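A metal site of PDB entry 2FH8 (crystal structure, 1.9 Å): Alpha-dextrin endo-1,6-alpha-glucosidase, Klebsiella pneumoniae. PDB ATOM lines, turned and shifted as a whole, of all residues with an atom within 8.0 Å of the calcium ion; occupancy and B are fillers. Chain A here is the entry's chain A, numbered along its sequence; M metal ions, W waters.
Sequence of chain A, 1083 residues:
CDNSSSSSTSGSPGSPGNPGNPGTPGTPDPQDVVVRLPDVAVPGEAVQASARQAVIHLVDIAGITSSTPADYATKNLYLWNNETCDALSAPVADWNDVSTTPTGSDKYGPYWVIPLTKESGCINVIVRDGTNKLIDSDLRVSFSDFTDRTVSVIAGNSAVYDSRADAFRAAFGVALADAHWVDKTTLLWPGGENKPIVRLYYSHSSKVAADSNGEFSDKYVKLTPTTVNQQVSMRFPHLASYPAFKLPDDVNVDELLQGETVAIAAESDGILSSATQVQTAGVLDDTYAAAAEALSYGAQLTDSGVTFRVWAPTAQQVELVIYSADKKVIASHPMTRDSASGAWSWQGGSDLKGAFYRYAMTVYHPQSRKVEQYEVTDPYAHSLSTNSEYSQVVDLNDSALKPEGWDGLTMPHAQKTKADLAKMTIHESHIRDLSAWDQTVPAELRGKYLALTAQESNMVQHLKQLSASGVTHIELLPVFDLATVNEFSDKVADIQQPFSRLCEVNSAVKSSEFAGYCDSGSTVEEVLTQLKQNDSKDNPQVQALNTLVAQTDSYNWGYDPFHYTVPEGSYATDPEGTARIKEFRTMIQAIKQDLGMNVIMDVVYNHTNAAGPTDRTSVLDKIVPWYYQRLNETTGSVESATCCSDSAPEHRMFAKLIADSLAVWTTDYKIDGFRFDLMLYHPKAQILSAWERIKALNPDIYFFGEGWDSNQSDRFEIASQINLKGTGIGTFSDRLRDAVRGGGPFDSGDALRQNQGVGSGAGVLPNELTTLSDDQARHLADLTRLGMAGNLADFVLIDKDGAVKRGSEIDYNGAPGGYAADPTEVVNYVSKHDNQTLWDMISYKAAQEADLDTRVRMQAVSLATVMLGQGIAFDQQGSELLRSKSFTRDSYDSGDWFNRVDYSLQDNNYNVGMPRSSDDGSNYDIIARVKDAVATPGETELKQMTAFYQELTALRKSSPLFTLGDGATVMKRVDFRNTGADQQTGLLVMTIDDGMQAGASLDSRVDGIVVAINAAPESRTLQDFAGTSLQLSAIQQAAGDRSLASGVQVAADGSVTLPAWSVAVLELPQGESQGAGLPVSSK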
ATOM      1  N   LEU A 384      -1.366 -23.989  13.570  1.00  0.00           N
ATOM      2  CA  LEU A 384      -0.531 -25.176  13.734  1.00  0.00           C
ATOM      3  C   LEU A 384      -1.214 -26.467  13.299  1.00  0.00           C
ATOM      4  O   LEU A 384      -2.432 -26.507  13.136  1.00  0.00           O
ATOM      5  CB  LEU A 384      -0.177 -25.329  15.218  1.00  0.00           C
ATOM      6  CG  LEU A 384       0.630 -24.257  15.969  1.00  0.00           C
ATOM      7  CD1 LEU A 384       0.372 -24.385  17.476  1.00  0.00           C
ATOM      8  CD2 LEU A 384       2.102 -24.430  15.667  1.00  0.00           C
ATOM      9  N   SER A 385      -0.422 -27.517  13.103  1.00  0.00           N
ATOM     10  CA  SER A 385      -0.966 -28.812  12.748  1.00  0.00           C
ATOM     11  C   SER A 385      -1.275 -29.478  14.095  1.00  0.00           C
ATOM     12  O   SER A 385      -0.968 -28.925  15.148  1.00  0.00           O
ATOM     13  CB  SER A 385       0.060 -29.654  11.991  1.00  0.00           C
ATOM     14  OG  SER A 385       1.147 -29.997  12.844  1.00  0.00           O
ATOM     15  N   THR A 386      -1.882 -30.664  14.055  1.00  0.00           N
ATOM     16  CA  THR A 386      -2.207 -31.370  15.294  1.00  0.00           C
ATOM     17  C   THR A 386      -0.991 -31.561  16.197  1.00  0.00           C
ATOM     18  O   THR A 386       0.068 -31.984  15.755  1.00  0.00           O
ATOM     19  CB  THR A 386      -2.806 -32.756  14.978  1.00  0.00           C
ATOM     20  OG1 THR A 386      -3.981 -32.598  14.182  1.00  0.00           O
ATOM     21  CG2 THR A 386      -3.182 -33.480  16.285  1.00  0.00           C
ATOM     22  N   ASN A 387      -1.167 -31.250  17.481  1.00  0.00           N
ATOM     23  CA  ASN A 387      -0.132 -31.356  18.511  1.00  0.00           C
ATOM     24  C   ASN A 387       1.055 -30.411  18.301  1.00  0.00           C
ATOM     25  O   ASN A 387       2.131 -30.627  18.862  1.00  0.00           O
ATOM     26  CB  ASN A 387       0.372 -32.797  18.635  1.00  0.00           C
ATOM     27  CG  ASN A 387       0.719 -33.166  20.084  1.00  0.00           C
ATOM     28  OD1 ASN A 387       1.644 -33.934  20.348  1.00  0.00           O
ATOM     29  ND2 ASN A 387      -0.047 -32.625  21.030  1.00  0.00           N
ATOM     30  N   SER A 388       0.844 -29.378  17.485  1.00  0.00           N
ATOM     31  CA  SER A 388       1.850 -28.339  17.231  1.00  0.00           C
ATOM     32  C   SER A 388       3.159 -28.786  16.570  1.00  0.00           C
ATOM     33  O   SER A 388       4.181 -28.119  16.734  1.00  0.00           O
ATOM     34  CB  SER A 388       2.187 -27.624  18.546  1.00  0.00           C
ATOM     35  OG  SER A 388       1.033 -27.479  19.359  1.00  0.00           O
ATOM     36  N   PHE A 480      -4.389 -20.669  25.064  1.00  0.00           N
ATOM     37  CA  PHE A 480      -3.372 -20.496  24.027  1.00  0.00           C
ATOM     38  C   PHE A 480      -2.857 -21.930  23.877  1.00  0.00           C
ATOM     39  O   PHE A 480      -3.317 -22.818  24.596  1.00  0.00           O
ATOM     40  CB  PHE A 480      -2.274 -19.529  24.484  1.00  0.00           C
ATOM     41  CG  PHE A 480      -1.744 -19.834  25.859  1.00  0.00           C
ATOM     42  CD1 PHE A 480      -0.757 -20.809  26.044  1.00  0.00           C
ATOM     43  CD2 PHE A 480      -2.236 -19.157  26.968  1.00  0.00           C
ATOM     44  CE1 PHE A 480      -0.290 -21.104  27.324  1.00  0.00           C
ATOM     45  CE2 PHE A 480      -1.770 -19.440  28.253  1.00  0.00           C
ATOM     46  CZ  PHE A 480      -0.791 -20.426  28.429  1.00  0.00           C
ATOM     47  N   ASP A 481      -1.921 -22.175  22.958  1.00  0.00           N
ATOM     48  CA  ASP A 481      -1.445 -23.540  22.747  1.00  0.00           C
ATOM     49  C   ASP A 481      -0.602 -24.108  23.899  1.00  0.00           C
ATOM     50  O   ASP A 481       0.570 -23.752  24.050  1.00  0.00           O
ATOM     51  CB  ASP A 481      -0.663 -23.617  21.427  1.00  0.00           C
ATOM     52  CG  ASP A 481      -0.098 -25.009  21.149  1.00  0.00           C
ATOM     53  OD1 ASP A 481      -0.781 -26.004  21.429  1.00  0.00           O
ATOM     54  OD2 ASP A 481       1.036 -25.098  20.624  1.00  0.00           O
ATOM     55  N   LEU A 482      -1.207 -24.968  24.705  1.00  0.00           N
ATOM     56  CA  LEU A 482      -0.469 -25.586  25.807  1.00  0.00           C
ATOM     57  C   LEU A 482       0.222 -26.848  25.302  1.00  0.00           C
ATOM     58  O   LEU A 482      -0.105 -27.357  24.231  1.00  0.00           O
ATOM     59  CB  LEU A 482      -1.408 -25.924  26.981  1.00  0.00           C
ATOM     60  CG  LEU A 482      -2.740 -26.606  26.688  1.00  0.00           C
ATOM     61  CD1 LEU A 482      -2.917 -27.793  27.620  1.00  0.00           C
ATOM     62  CD2 LEU A 482      -3.852 -25.598  26.896  1.00  0.00           C
ATOM     63  N   ALA A 483       1.182 -27.341  26.079  1.00  0.00           N
ATOM     64  CA  ALA A 483       1.951 -28.510  25.664  1.00  0.00           C
ATOM     65  C   ALA A 483       1.589 -29.836  26.332  1.00  0.00           C
ATOM     66  O   ALA A 483       1.777 -30.898  25.748  1.00  0.00           O
ATOM     67  CB  ALA A 483       3.437 -28.233  25.892  1.00  0.00           C
ATOM     68  N   THR A 484       1.058 -29.759  27.543  1.00  0.00           N
ATOM     69  CA  THR A 484       0.733 -30.925  28.371  1.00  0.00           C
ATOM     70  C   THR A 484      -0.502 -31.788  28.112  1.00  0.00           C
ATOM     71  O   THR A 484      -0.952 -32.515  29.001  1.00  0.00           O
ATOM     72  CB  THR A 484       0.727 -30.525  29.849  1.00  0.00           C
ATOM     73  OG1 THR A 484      -0.062 -29.351  30.025  1.00  0.00           O
ATOM     74  CG2 THR A 484       2.142 -30.248  30.319  1.00  0.00           C
ATOM     75  N   VAL A 485      -1.038 -31.722  26.905  1.00  0.00           N
ATOM     76  CA  VAL A 485      -2.177 -32.545  26.518  1.00  0.00           C
ATOM     77  C   VAL A 485      -1.847 -32.959  25.091  1.00  0.00           C
ATOM     78  O   VAL A 485      -1.519 -32.110  24.267  1.00  0.00           O
ATOM     79  CB  VAL A 485      -3.508 -31.783  26.543  1.00  0.00           C
ATOM     80  CG1 VAL A 485      -4.595 -32.602  25.843  1.00  0.00           C
ATOM     81  CG2 VAL A 485      -3.934 -31.509  27.989  1.00  0.00           C
ATOM     82  N   ASN A 486      -1.882 -34.251  24.807  1.00  0.00           N
ATOM     83  CA  ASN A 486      -1.586 -34.707  23.456  1.00  0.00           C
ATOM     84  C   ASN A 486      -2.832 -34.429  22.629  1.00  0.00           C
ATOM     85  O   ASN A 486      -3.946 -34.806  23.008  1.00  0.00           O
ATOM     86  CB  ASN A 486      -1.282 -36.206  23.452  1.00  0.00           C
ATOM     87  CG  ASN A 486      -0.697 -36.672  22.133  1.00  0.00           C
ATOM     88  OD1 ASN A 486      -1.203 -36.330  21.065  1.00  0.00           O
ATOM     89  ND2 ASN A 486       0.386 -37.438  22.208  1.00  0.00           N
ATOM     90  N   GLU A 487      -2.661 -33.738  21.505  1.00  0.00           N
ATOM     91  CA  GLU A 487      -3.794 -33.392  20.653  1.00  0.00           C
ATOM     92  C   GLU A 487      -4.207 -34.491  19.670  1.00  0.00           C
ATOM     93  O   GLU A 487      -5.184 -34.346  18.949  1.00  0.00           O
ATOM     94  CB  GLU A 487      -3.517 -32.081  19.928  1.00  0.00           C
ATOM     95  CG  GLU A 487      -3.180 -30.943  20.893  1.00  0.00           C
ATOM     96  CD  GLU A 487      -3.023 -29.606  20.207  1.00  0.00           C
ATOM     97  OE1 GLU A 487      -2.790 -29.589  18.979  1.00  0.00           O
ATOM     98  OE2 GLU A 487      -3.125 -28.567  20.902  1.00  0.00           O
ATOM     99  N   ASP A 560       1.393 -24.185  30.633  1.00  0.00           N
ATOM    100  CA  ASP A 560       2.592 -24.719  30.008  1.00  0.00           C
ATOM    101  C   ASP A 560       2.664 -24.308  28.534  1.00  0.00           C
ATOM    102  O   ASP A 560       2.355 -25.104  27.640  1.00  0.00           O
ATOM    103  CB  ASP A 560       2.615 -26.239  30.121  1.00  0.00           C
ATOM    104  CG  ASP A 560       2.241 -26.733  31.502  1.00  0.00           C
ATOM    105  OD1 ASP A 560       1.052 -27.001  31.746  1.00  0.00           O
ATOM    106  OD2 ASP A 560       3.153 -26.839  32.354  1.00  0.00           O
ATOM    107  N   PRO A 561       3.073 -23.062  28.273  1.00  0.00           N
ATOM    108  CA  PRO A 561       3.200 -22.484  26.927  1.00  0.00           C
ATOM    109  C   PRO A 561       4.043 -23.257  25.909  1.00  0.00           C
ATOM    110  O   PRO A 561       5.226 -23.542  26.145  1.00  0.00           O
ATOM    111  CB  PRO A 561       3.790 -21.103  27.217  1.00  0.00           C
ATOM    112  CG  PRO A 561       3.193 -20.760  28.550  1.00  0.00           C
ATOM    113  CD  PRO A 561       3.333 -22.053  29.309  1.00  0.00           C
ATOM    114  N   PHE A 562       3.434 -23.572  24.771  1.00  0.00           N
ATOM    115  CA  PHE A 562       4.105 -24.257  23.667  1.00  0.00           C
ATOM    116  C   PHE A 562       4.221 -23.162  22.593  1.00  0.00           C
ATOM    117  O   PHE A 562       5.302 -22.913  22.055  1.00  0.00           O
ATOM    118  CB  PHE A 562       3.248 -25.420  23.162  1.00  0.00           C
ATOM    119  CG  PHE A 562       3.998 -26.439  22.345  1.00  0.00           C
ATOM    120  CD1 PHE A 562       3.415 -27.680  22.054  1.00  0.00           C
ATOM    121  CD2 PHE A 562       5.260 -26.169  21.835  1.00  0.00           C
ATOM    122  CE1 PHE A 562       4.081 -28.627  21.284  1.00  0.00           C
ATOM    123  CE2 PHE A 562       5.942 -27.111  21.058  1.00  0.00           C
ATOM    124  CZ  PHE A 562       5.351 -28.345  20.784  1.00  0.00           C
ATOM    125  N   HIS A 563       3.098 -22.506  22.311  1.00  0.00           N
ATOM    126  CA  HIS A 563       3.036 -21.395  21.361  1.00  0.00           C
ATOM    127  C   HIS A 563       2.091 -20.375  21.966  1.00  0.00           C
ATOM    128  O   HIS A 563       0.936 -20.679  22.266  1.00  0.00           O
ATOM    129  CB  HIS A 563       2.518 -21.854  19.997  1.00  0.00           C
ATOM    130  CG  HIS A 563       3.417 -22.846  19.334  1.00  0.00           C
ATOM    131  ND1 HIS A 563       4.445 -22.470  18.497  1.00  0.00           N
ATOM    132  CD2 HIS A 563       3.474 -24.199  19.422  1.00  0.00           C
ATOM    133  CE1 HIS A 563       5.093 -23.556  18.093  1.00  0.00           C
ATOM    134  NE2 HIS A 563       4.521 -24.606  18.643  1.00  0.00           N
ATOM    135  N   VAL A 566      -1.539 -18.988  19.368  1.00  0.00           N
ATOM    136  CA  VAL A 566      -2.366 -19.932  18.621  1.00  0.00           C
ATOM    137  C   VAL A 566      -3.286 -20.568  19.666  1.00  0.00           C
ATOM    138  O   VAL A 566      -2.837 -20.895  20.760  1.00  0.00           O
ATOM    139  CB  VAL A 566      -1.518 -21.054  17.982  1.00  0.00           C
ATOM    140  CG1 VAL A 566      -2.405 -21.935  17.105  1.00  0.00           C
ATOM    141  CG2 VAL A 566      -0.390 -20.468  17.178  1.00  0.00           C
ATOM    142  N   PRO A 567      -4.580 -20.725  19.342  1.00  0.00           N
ATOM    143  CA  PRO A 567      -5.489 -21.335  20.308  1.00  0.00           C
ATOM    144  C   PRO A 567      -5.067 -22.785  20.565  1.00  0.00           C
ATOM    145  O   PRO A 567      -4.414 -23.397  19.705  1.00  0.00           O
ATOM    146  CB  PRO A 567      -6.851 -21.266  19.607  1.00  0.00           C
ATOM    147  CG  PRO A 567      -6.726 -20.035  18.763  1.00  0.00           C
ATOM    148  CD  PRO A 567      -5.326 -20.174  18.195  1.00  0.00           C
ATOM    149  N   GLU A 568      -5.396 -23.314  21.744  1.00  0.00           N
ATOM    150  CA  GLU A 568      -5.064 -24.690  22.080  1.00  0.00           C
ATOM    151  C   GLU A 568      -5.836 -25.606  21.130  1.00  0.00           C
ATOM    152  O   GLU A 568      -6.988 -25.323  20.814  1.00  0.00           O
ATOM    153  CB  GLU A 568      -5.453 -24.992  23.534  1.00  0.00           C
ATOM    154  CG  GLU A 568      -5.594 -26.484  23.855  1.00  0.00           C
ATOM    155  CD  GLU A 568      -4.318 -27.283  23.665  1.00  0.00           C
ATOM    156  OE1 GLU A 568      -4.386 -28.533  23.754  1.00  0.00           O
ATOM    157  OE2 GLU A 568      -3.241 -26.684  23.431  1.00  0.00           O
ATOM    158  N   GLY A 569      -5.213 -26.686  20.688  1.00  0.00           N
ATOM    159  CA  GLY A 569      -5.879 -27.584  19.756  1.00  0.00           C
ATOM    160  C   GLY A 569      -6.845 -28.604  20.345  1.00  0.00           C
ATOM    161  O   GLY A 569      -7.876 -28.900  19.730  1.00  0.00           O
ATOM    162  N   SER A 570      -6.541 -29.131  21.535  1.00  0.00           N
ATOM    163  CA  SER A 570      -7.415 -30.137  22.149  1.00  0.00           C
ATOM    164  C   SER A 570      -8.820 -29.647  22.445  1.00  0.00           C
ATOM    165  O   SER A 570      -9.734 -30.467  22.618  1.00  0.00           O
ATOM    166  CB  SER A 570      -6.795 -30.685  23.426  1.00  0.00           C
ATOM    167  OG  SER A 570      -6.803 -29.717  24.463  1.00  0.00           O
ATOM    168  N   TYR A 571      -9.007 -28.332  22.529  1.00  0.00           N
ATOM    169  CA  TYR A 571     -10.331 -27.783  22.812  1.00  0.00           C
ATOM    170  C   TYR A 571     -11.144 -27.557  21.543  1.00  0.00           C
ATOM    171  O   TYR A 571     -12.286 -27.080  21.598  1.00  0.00           O
ATOM    172  CB  TYR A 571     -10.227 -26.461  23.594  1.00  0.00           C
ATOM    173  CG  TYR A 571      -9.560 -26.584  24.948  1.00  0.00           C
ATOM    174  CD1 TYR A 571      -9.854 -27.651  25.805  1.00  0.00           C
ATOM    175  CD2 TYR A 571      -8.626 -25.639  25.387  1.00  0.00           C
ATOM    176  CE1 TYR A 571      -9.255 -27.766  27.053  1.00  0.00           C
ATOM    177  CE2 TYR A 571      -8.020 -25.743  26.644  1.00  0.00           C
ATOM    178  CZ  TYR A 571      -8.332 -26.815  27.471  1.00  0.00           C
ATOM    179  OH  TYR A 571      -7.743 -26.951  28.711  1.00  0.00           O
ATOM    180  N   PRO A 575      -8.258 -30.498  15.588  1.00  0.00           N
ATOM    181  CA  PRO A 575      -6.965 -29.872  15.875  1.00  0.00           C
ATOM    182  C   PRO A 575      -6.017 -29.705  14.688  1.00  0.00           C
ATOM    183  O   PRO A 575      -4.940 -29.126  14.835  1.00  0.00           O
ATOM    184  CB  PRO A 575      -6.377 -30.799  16.929  1.00  0.00           C
ATOM    185  CG  PRO A 575      -6.789 -32.134  16.402  1.00  0.00           C
ATOM    186  CD  PRO A 575      -8.245 -31.920  15.998  1.00  0.00           C
ATOM    187  N   ARG A 580      -9.425 -24.761  14.295  1.00  0.00           N
ATOM    188  CA  ARG A 580      -9.579 -24.276  15.665  1.00  0.00           C
ATOM    189  C   ARG A 580      -9.779 -22.774  15.776  1.00  0.00           C
ATOM    190  O   ARG A 580     -10.413 -22.295  16.717  1.00  0.00           O
ATOM    191  CB  ARG A 580      -8.369 -24.681  16.508  1.00  0.00           C
ATOM    192  CG  ARG A 580      -7.143 -23.805  16.253  1.00  0.00           C
ATOM    193  CD  ARG A 580      -5.937 -24.296  17.062  1.00  0.00           C
ATOM    194  NE  ARG A 580      -5.352 -25.516  16.487  1.00  0.00           N
ATOM    195  CZ  ARG A 580      -4.225 -26.049  16.919  1.00  0.00           C
ATOM    196  NH1 ARG A 580      -3.559 -25.488  17.922  1.00  0.00           N
ATOM    197  NH2 ARG A 580      -3.732 -27.136  16.335  1.00  0.00           N
ATOM    198  N   ARG A 616      10.999 -31.612  22.890  1.00  0.00           N
ATOM    199  CA  ARG A 616       9.989 -31.403  21.860  1.00  0.00           C
ATOM    200  C   ARG A 616       9.367 -30.014  21.944  1.00  0.00           C
ATOM    201  O   ARG A 616       9.183 -29.347  20.926  1.00  0.00           O
ATOM    202  CB  ARG A 616       8.895 -32.470  22.015  1.00  0.00           C
ATOM    203  CG  ARG A 616       7.703 -32.331  21.075  1.00  0.00           C
ATOM    204  CD  ARG A 616       6.592 -33.329  21.428  1.00  0.00           C
ATOM    205  NE  ARG A 616       6.026 -33.076  22.746  1.00  0.00           N
ATOM    206  CZ  ARG A 616       4.853 -32.482  22.972  1.00  0.00           C
ATOM    207  NH1 ARG A 616       4.112 -32.076  21.954  1.00  0.00           N
ATOM    208  NH2 ARG A 616       4.433 -32.285  24.216  1.00  0.00           N
HETATM  209 CA    CA M   1      -1.483 -27.875  22.499  1.00  0.00          CA
HETATM  210  O   HOH W   1      -2.157 -29.594  24.004  1.00  0.00           O
HETATM  211  O   HOH W   2       0.002 -29.153  21.418  1.00  0.00           O
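Water W2 bridges OG of Ser 388 (2.8 Å) and ND2 of Asn 387 (3.5 Å).
Water W1 bridges OE1 of Glu 568 (2.5 Å) and O of Val 485 (2.6 Å).
The calcium ion is bound by water W2 (2.2 Å), the side-chain carboxylate of Asp 481 (2.3 Å), the backbone carbonyl oxygen of Leu 482 (2.3 Å), the side-chain carboxylate of Glu 568 (2.3 Å), water W1 (2.4 Å) and the side-chain carboxylate of Glu 487 (2.4 Å).
OD2 of Asp 481 sits at hydrogen-bond distance from OG of Ser 388.
O of Asp 481 sits at hydrogen-bond distance from N of Phe 562 (3.0 Å).
The backbone carbonyl oxygen (O) of His 563 lies within hydrogen-bond range of the backbone NH (N) of Asp 481 (3.3 Å).
N of Asp 481 sits at hydrogen-bond distance from O of Val 566 (2.7 Å).
The side-chain hydroxyl (OG) of Ser 570 lies within hydrogen-bond range of the side-chain carboxylate (OE1) of Glu 568 (2.8 Å).
N of Gly 569 sits close to OE2 of Glu 487 (2.8 Å).
The side-chain carboxylate (OE1) of Glu 487 sits at hydrogen-bond distance from the backbone NH (N) of Asn 387 (2.8 Å).
The guanidinium group of Arg 580 is in salt-bridge range of the side-chain carboxylate of Glu 487, 3.7 Å away.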
